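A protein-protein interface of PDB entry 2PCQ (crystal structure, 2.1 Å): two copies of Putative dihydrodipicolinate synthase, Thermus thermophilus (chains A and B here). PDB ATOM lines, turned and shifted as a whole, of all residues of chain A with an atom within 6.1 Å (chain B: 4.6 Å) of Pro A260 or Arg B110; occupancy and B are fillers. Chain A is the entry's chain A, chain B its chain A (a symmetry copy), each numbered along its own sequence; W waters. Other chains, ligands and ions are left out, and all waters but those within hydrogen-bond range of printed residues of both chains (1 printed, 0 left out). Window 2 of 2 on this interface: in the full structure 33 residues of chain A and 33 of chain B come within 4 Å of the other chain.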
ATOM      1  N   PRO A 239      -0.092  13.850 -21.807  1.00  0.00           N
ATOM      2  CA  PRO A 239      -0.445  13.872 -20.383  1.00  0.00           C
ATOM      3  C   PRO A 239      -0.242  12.511 -19.711  1.00  0.00           C
ATOM      4  O   PRO A 239       0.243  12.439 -18.583  1.00  0.00           O
ATOM      5  CB  PRO A 239      -1.913  14.297 -20.395  1.00  0.00           C
ATOM      6  CG  PRO A 239      -1.991  15.180 -21.607  1.00  0.00           C
ATOM      7  CD  PRO A 239      -1.189  14.394 -22.628  1.00  0.00           C
ATOM      8  N   TYR A 254       5.045  18.397 -16.200  1.00  0.00           N
ATOM      9  CA  TYR A 254       3.647  18.411 -16.626  1.00  0.00           C
ATOM     10  C   TYR A 254       3.451  19.031 -18.001  1.00  0.00           C
ATOM     11  O   TYR A 254       4.291  19.796 -18.476  1.00  0.00           O
ATOM     12  CB  TYR A 254       2.820  19.213 -15.618  1.00  0.00           C
ATOM     13  CG  TYR A 254       2.991  18.744 -14.196  1.00  0.00           C
ATOM     14  CD1 TYR A 254       2.077  17.870 -13.615  1.00  0.00           C
ATOM     15  CD2 TYR A 254       4.098  19.138 -13.445  1.00  0.00           C
ATOM     16  CE1 TYR A 254       2.260  17.397 -12.320  1.00  0.00           C
ATOM     17  CE2 TYR A 254       4.294  18.673 -12.154  1.00  0.00           C
ATOM     18  CZ  TYR A 254       3.374  17.803 -11.598  1.00  0.00           C
ATOM     19  OH  TYR A 254       3.573  17.336 -10.321  1.00  0.00           O
ATOM     20  N   PRO A 255       2.329  18.705 -18.662  1.00  0.00           N
ATOM     21  CA  PRO A 255       2.055  19.269 -19.987  1.00  0.00           C
ATOM     22  C   PRO A 255       1.871  20.775 -19.800  1.00  0.00           C
ATOM     23  O   PRO A 255       1.415  21.218 -18.745  1.00  0.00           O
ATOM     24  CB  PRO A 255       0.752  18.581 -20.392  1.00  0.00           C
ATOM     25  CG  PRO A 255       0.827  17.261 -19.677  1.00  0.00           C
ATOM     26  CD  PRO A 255       1.342  17.669 -18.317  1.00  0.00           C
ATOM     27  N   ARG A 256       2.215  21.565 -20.806  1.00  0.00           N
ATOM     28  CA  ARG A 256       2.069  23.007 -20.673  1.00  0.00           C
ATOM     29  C   ARG A 256       0.594  23.400 -20.728  1.00  0.00           C
ATOM     30  O   ARG A 256      -0.143  22.925 -21.590  1.00  0.00           O
ATOM     31  CB  ARG A 256       2.857  23.724 -21.776  1.00  0.00           C
ATOM     32  CG  ARG A 256       3.335  25.102 -21.361  1.00  0.00           C
ATOM     33  CD  ARG A 256       4.340  25.711 -22.338  1.00  0.00           C
ATOM     34  NE  ARG A 256       5.200  26.652 -21.626  1.00  0.00           N
ATOM     35  CZ  ARG A 256       6.087  27.467 -22.187  1.00  0.00           C
ATOM     36  NH1 ARG A 256       6.261  27.489 -23.502  1.00  0.00           N
ATOM     37  NH2 ARG A 256       6.818  28.261 -21.415  1.00  0.00           N
ATOM     38  N   PRO A 258      -2.911  25.054 -21.569  1.00  0.00           N
ATOM     39  CA  PRO A 258      -4.074  24.502 -20.868  1.00  0.00           C
ATOM     40  C   PRO A 258      -4.215  22.981 -20.788  1.00  0.00           C
ATOM     41  O   PRO A 258      -5.255  22.484 -20.364  1.00  0.00           O
ATOM     42  CB  PRO A 258      -5.230  25.120 -21.628  1.00  0.00           C
ATOM     43  CG  PRO A 258      -4.736  24.991 -23.047  1.00  0.00           C
ATOM     44  CD  PRO A 258      -3.281  25.438 -22.947  1.00  0.00           C
ATOM     45  N   TYR A 259      -3.199  22.237 -21.197  1.00  0.00           N
ATOM     46  CA  TYR A 259      -3.315  20.787 -21.136  1.00  0.00           C
ATOM     47  C   TYR A 259      -3.313  20.283 -19.688  1.00  0.00           C
ATOM     48  O   TYR A 259      -2.652  20.855 -18.820  1.00  0.00           O
ATOM     49  CB  TYR A 259      -2.218  20.141 -21.984  1.00  0.00           C
ATOM     50  CG  TYR A 259      -2.455  20.372 -23.467  1.00  0.00           C
ATOM     51  CD1 TYR A 259      -1.897  21.470 -24.129  1.00  0.00           C
ATOM     52  CD2 TYR A 259      -3.292  19.524 -24.193  1.00  0.00           C
ATOM     53  CE1 TYR A 259      -2.172  21.715 -25.479  1.00  0.00           C
ATOM     54  CE2 TYR A 259      -3.575  19.761 -25.536  1.00  0.00           C
ATOM     55  CZ  TYR A 259      -3.011  20.853 -26.174  1.00  0.00           C
ATOM     56  OH  TYR A 259      -3.283  21.068 -27.505  1.00  0.00           O
ATOM     57  N   PRO A 260      -4.070  19.205 -19.412  1.00  0.00           N
ATOM     58  CA  PRO A 260      -4.206  18.594 -18.086  1.00  0.00           C
ATOM     59  C   PRO A 260      -2.965  17.962 -17.472  1.00  0.00           C
ATOM     60  O   PRO A 260      -2.197  17.271 -18.146  1.00  0.00           O
ATOM     61  CB  PRO A 260      -5.330  17.584 -18.295  1.00  0.00           C
ATOM     62  CG  PRO A 260      -5.061  17.100 -19.684  1.00  0.00           C
ATOM     63  CD  PRO A 260      -4.765  18.392 -20.428  1.00  0.00           C
ATOM     64  N   ALA A 261      -2.788  18.199 -16.175  1.00  0.00           N
ATOM     65  CA  ALA A 261      -1.656  17.663 -15.428  1.00  0.00           C
ATOM     66  C   ALA A 261      -1.777  16.149 -15.273  1.00  0.00           C
ATOM     67  O   ALA A 261      -0.777  15.443 -15.130  1.00  0.00           O
ATOM     68  CB  ALA A 261      -1.584  18.323 -14.054  1.00  0.00           C
ATOM     69  N   GLU A 262      -3.010  15.658 -15.302  1.00  0.00           N
ATOM     70  CA  GLU A 262      -3.269  14.234 -15.170  1.00  0.00           C
ATOM     71  C   GLU A 262      -4.160  13.730 -16.300  1.00  0.00           C
ATOM     72  O   GLU A 262      -5.013  14.462 -16.804  1.00  0.00           O
ATOM     73  CB  GLU A 262      -3.907  13.952 -13.808  1.00  0.00           C
ATOM     74  CG  GLU A 262      -2.915  14.043 -12.656  1.00  0.00           C
ATOM     75  CD  GLU A 262      -3.569  13.921 -11.290  1.00  0.00           C
ATOM     76  OE1 GLU A 262      -4.584  13.203 -11.167  1.00  0.00           O
ATOM     77  OE2 GLU A 262      -3.053  14.534 -10.332  1.00  0.00           O
ATOM     78  N   SER A 263      -3.949  12.479 -16.698  1.00  0.00           N
ATOM     79  CA  SER A 263      -4.717  11.866 -17.777  1.00  0.00           C
ATOM     80  C   SER A 263      -5.963  11.124 -17.301  1.00  0.00           C
ATOM     81  O   SER A 263      -5.942  10.452 -16.268  1.00  0.00           O
ATOM     82  CB  SER A 263      -3.829  10.890 -18.555  1.00  0.00           C
ATOM     83  OG  SER A 263      -4.599  10.099 -19.449  1.00  0.00           O
ATOM     84  N   PRO A 264      -7.067  11.232 -18.058  1.00  0.00           N
ATOM     85  CA  PRO A 264      -8.329  10.563 -17.720  1.00  0.00           C
ATOM     86  C   PRO A 264      -8.176   9.040 -17.820  1.00  0.00           C
ATOM     87  O   PRO A 264      -9.033   8.285 -17.364  1.00  0.00           O
ATOM     88  CB  PRO A 264      -9.302  11.098 -18.775  1.00  0.00           C
ATOM     89  CG  PRO A 264      -8.729  12.432 -19.137  1.00  0.00           C
ATOM     90  CD  PRO A 264      -7.253  12.146 -19.202  1.00  0.00           C
ATOM     91  N   SER B 103      -5.931  15.727 -26.829  1.00  0.00           N
ATOM     92  CA  SER B 103      -5.696  15.546 -25.397  1.00  0.00           C
ATOM     93  C   SER B 103      -6.118  16.764 -24.577  1.00  0.00           C
ATOM     94  O   SER B 103      -5.984  16.774 -23.351  1.00  0.00           O
ATOM     95  CB  SER B 103      -4.212  15.271 -25.143  1.00  0.00           C
ATOM     96  OG  SER B 103      -3.769  14.130 -25.862  1.00  0.00           O
ATOM     97  N   LEU B 104      -6.628  17.785 -25.258  1.00  0.00           N
ATOM     98  CA  LEU B 104      -7.042  19.023 -24.605  1.00  0.00           C
ATOM     99  C   LEU B 104      -8.175  18.859 -23.585  1.00  0.00           C
ATOM    100  O   LEU B 104      -8.091  19.377 -22.472  1.00  0.00           O
ATOM    101  CB  LEU B 104      -7.436  20.044 -25.675  1.00  0.00           C
ATOM    102  CG  LEU B 104      -7.623  21.510 -25.288  1.00  0.00           C
ATOM    103  CD1 LEU B 104      -6.380  22.034 -24.579  1.00  0.00           C
ATOM    104  CD2 LEU B 104      -7.897  22.317 -26.552  1.00  0.00           C
ATOM    105  N   ALA B 106     -11.278  19.390 -21.340  1.00  0.00           N
ATOM    106  CA  ALA B 106     -11.884  20.606 -20.808  1.00  0.00           C
ATOM    107  C   ALA B 106     -10.889  21.762 -20.842  1.00  0.00           C
ATOM    108  O   ALA B 106     -11.231  22.893 -20.496  1.00  0.00           O
ATOM    109  CB  ALA B 106     -12.370  20.371 -19.378  1.00  0.00           C
ATOM    110  N   GLY B 107      -9.658  21.468 -21.252  1.00  0.00           N
ATOM    111  CA  GLY B 107      -8.640  22.501 -21.345  1.00  0.00           C
ATOM    112  C   GLY B 107      -9.015  23.545 -22.387  1.00  0.00           C
ATOM    113  O   GLY B 107      -8.470  24.650 -22.394  1.00  0.00           O
ATOM    114  N   LEU B 108      -9.942  23.194 -23.275  1.00  0.00           N
ATOM    115  CA  LEU B 108     -10.397  24.122 -24.307  1.00  0.00           C
ATOM    116  C   LEU B 108     -11.078  25.311 -23.644  1.00  0.00           C
ATOM    117  O   LEU B 108     -10.820  26.464 -23.994  1.00  0.00           O
ATOM    118  CB  LEU B 108     -11.390  23.442 -25.254  1.00  0.00           C
ATOM    119  CG  LEU B 108     -12.000  24.349 -26.333  1.00  0.00           C
ATOM    120  CD1 LEU B 108     -10.921  24.800 -27.304  1.00  0.00           C
ATOM    121  CD2 LEU B 108     -13.085  23.597 -27.072  1.00  0.00           C
ATOM    122  N   LEU B 109     -11.959  25.018 -22.691  1.00  0.00           N
ATOM    123  CA  LEU B 109     -12.678  26.062 -21.972  1.00  0.00           C
ATOM    124  C   LEU B 109     -11.701  26.847 -21.104  1.00  0.00           C
ATOM    125  O   LEU B 109     -11.790  28.070 -21.015  1.00  0.00           O
ATOM    126  CB  LEU B 109     -13.781  25.447 -21.099  1.00  0.00           C
ATOM    127  CG  LEU B 109     -14.826  24.607 -21.842  1.00  0.00           C
ATOM    128  CD1 LEU B 109     -15.819  24.022 -20.851  1.00  0.00           C
ATOM    129  CD2 LEU B 109     -15.540  25.474 -22.872  1.00  0.00           C
ATOM    130  N   ARG B 110     -10.768  26.142 -20.468  1.00  0.00           N
ATOM    131  CA  ARG B 110      -9.781  26.804 -19.622  1.00  0.00           C
ATOM    132  C   ARG B 110      -8.955  27.787 -20.442  1.00  0.00           C
ATOM    133  O   ARG B 110      -8.610  28.868 -19.964  1.00  0.00           O
ATOM    134  CB  ARG B 110      -8.844  25.782 -18.966  1.00  0.00           C
ATOM    135  CG  ARG B 110      -9.519  24.858 -17.962  1.00  0.00           C
ATOM    136  CD  ARG B 110      -8.491  24.208 -17.040  1.00  0.00           C
ATOM    137  NE  ARG B 110      -7.606  23.266 -17.726  1.00  0.00           N
ATOM    138  CZ  ARG B 110      -7.936  22.017 -18.041  1.00  0.00           C
ATOM    139  NH1 ARG B 110      -9.138  21.547 -17.734  1.00  0.00           N
ATOM    140  NH2 ARG B 110      -7.059  21.233 -18.659  1.00  0.00           N
ATOM    141  N   TYR B 111      -8.641  27.407 -21.676  1.00  0.00           N
ATOM    142  CA  TYR B 111      -7.847  28.256 -22.559  1.00  0.00           C
ATOM    143  C   TYR B 111      -8.561  29.583 -22.828  1.00  0.00           C
ATOM    144  O   TYR B 111      -8.017  30.657 -22.576  1.00  0.00           O
ATOM    145  CB  TYR B 111      -7.587  27.532 -23.885  1.00  0.00           C
ATOM    146  CG  TYR B 111      -6.668  28.271 -24.834  1.00  0.00           C
ATOM    147  CD1 TYR B 111      -5.315  28.451 -24.535  1.00  0.00           C
ATOM    148  CD2 TYR B 111      -7.152  28.800 -26.031  1.00  0.00           C
ATOM    149  CE1 TYR B 111      -4.468  29.139 -25.406  1.00  0.00           C
ATOM    150  CE2 TYR B 111      -6.314  29.489 -26.907  1.00  0.00           C
ATOM    151  CZ  TYR B 111      -4.977  29.656 -26.588  1.00  0.00           C
ATOM    152  OH  TYR B 111      -4.157  30.338 -27.452  1.00  0.00           O
ATOM    153  N   TYR B 112      -9.785  29.501 -23.333  1.00  0.00           N
ATOM    154  CA  TYR B 112     -10.559  30.691 -23.647  1.00  0.00           C
ATOM    155  C   TYR B 112     -10.926  31.537 -22.430  1.00  0.00           C
ATOM    156  O   TYR B 112     -10.941  32.762 -22.507  1.00  0.00           O
ATOM    157  CB  TYR B 112     -11.825  30.303 -24.413  1.00  0.00           C
ATOM    158  CG  TYR B 112     -11.569  29.980 -25.868  1.00  0.00           C
ATOM    159  CD1 TYR B 112     -11.797  28.699 -26.374  1.00  0.00           C
ATOM    160  CD2 TYR B 112     -11.096  30.958 -26.743  1.00  0.00           C
ATOM    161  CE1 TYR B 112     -11.561  28.403 -27.718  1.00  0.00           C
ATOM    162  CE2 TYR B 112     -10.858  30.673 -28.085  1.00  0.00           C
ATOM    163  CZ  TYR B 112     -11.094  29.397 -28.566  1.00  0.00           C
ATOM    164  OH  TYR B 112     -10.881  29.120 -29.896  1.00  0.00           O
ATOM    165  N   GLU B 113     -11.222  30.892 -21.307  1.00  0.00           N
ATOM    166  CA  GLU B 113     -11.582  31.635 -20.106  1.00  0.00           C
ATOM    167  C   GLU B 113     -10.380  32.407 -19.579  1.00  0.00           C
ATOM    168  O   GLU B 113     -10.525  33.511 -19.064  1.00  0.00           O
ATOM    169  CB  GLU B 113     -12.131  30.684 -19.041  1.00  0.00           C
ATOM    170  CG  GLU B 113     -13.394  29.968 -19.498  1.00  0.00           C
ATOM    171  CD  GLU B 113     -13.906  28.965 -18.489  1.00  0.00           C
ATOM    172  OE1 GLU B 113     -13.105  28.487 -17.660  1.00  0.00           O
ATOM    173  OE2 GLU B 113     -15.111  28.640 -18.541  1.00  0.00           O
ATOM    174  N   ALA B 114      -9.189  31.833 -19.729  1.00  0.00           N
ATOM    175  CA  ALA B 114      -7.974  32.498 -19.280  1.00  0.00           C
ATOM    176  C   ALA B 114      -7.740  33.753 -20.121  1.00  0.00           C
ATOM    177  O   ALA B 114      -7.439  34.822 -19.588  1.00  0.00           O
ATOM    178  CB  ALA B 114      -6.786  31.559 -19.402  1.00  0.00           C
HETATM  179  O   HOH W   1      -5.304  24.829 -17.834  1.00  0.00           O
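Printed residues of chain B that touch a printed residue of chain A: Ser B103, Leu B104, Gly B107, Arg B110 and Tyr B111.
Of the 11 printed residues of chain A, 3 touch a printed residue of chain B.
Hydrophobic or aromatic side chains of chain A within 4 Å of the printed part of chain B: Pro A258, Tyr A259 and Pro A260.
Among the printed residues, 9 pairs touch across the chains.
Among the printed residues, no Asp or Glu carboxylate lies within 4 Å of a Lys or Arg side-chain nitrogen of the other chain.
Among the printed residues, pairs that only touch across the chains: Pro A258 with Gly B107, Pro A260 with Ser B103, Tyr A259 with Leu B104, Pro A260 with Arg B110, Pro A258 with Leu B104, Pro A258 with Tyr B111, Tyr A259 with Ser B103 and Tyr A259 with Arg B110.
O of Pro A258 is in hydrogen-bond range of NH2 of Arg B110 (2.8 Å).
Water W1 lies within hydrogen-bond range of NE of Arg B110 (2.8 Å) and O of Pro A258 (3.4 Å).
Pro A260 touches just these residues of chain B: Ser B103 and Arg B110.
Printed residues of chain A within 4 Å of Arg B110: Pro A258, Tyr A259 and Pro A260.
Printed residues of chain A within 4 Å of Ser B103: Tyr A259 and Pro A260.
Printed residues of chain A within 4 Å of Leu B104: Pro A258 and Tyr A259.
Printed residues of chain B within 4 Å of Tyr A259: Ser B103 (3.9 Å), Leu B104 (3.6 Å) and Arg B110 (3.999 Å).
The nearest residue of chain B that does not touch Pro A260 is Leu B104 (4.03 Å).
The nearest printed residue of chain A that does not touch Gly B107 is Tyr A259 (5.4 Å).
No position is printed for both chains.
Of the 9 pairs that touch across the chains among the printed residues, none has its exchanged pair printed and touching as well.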
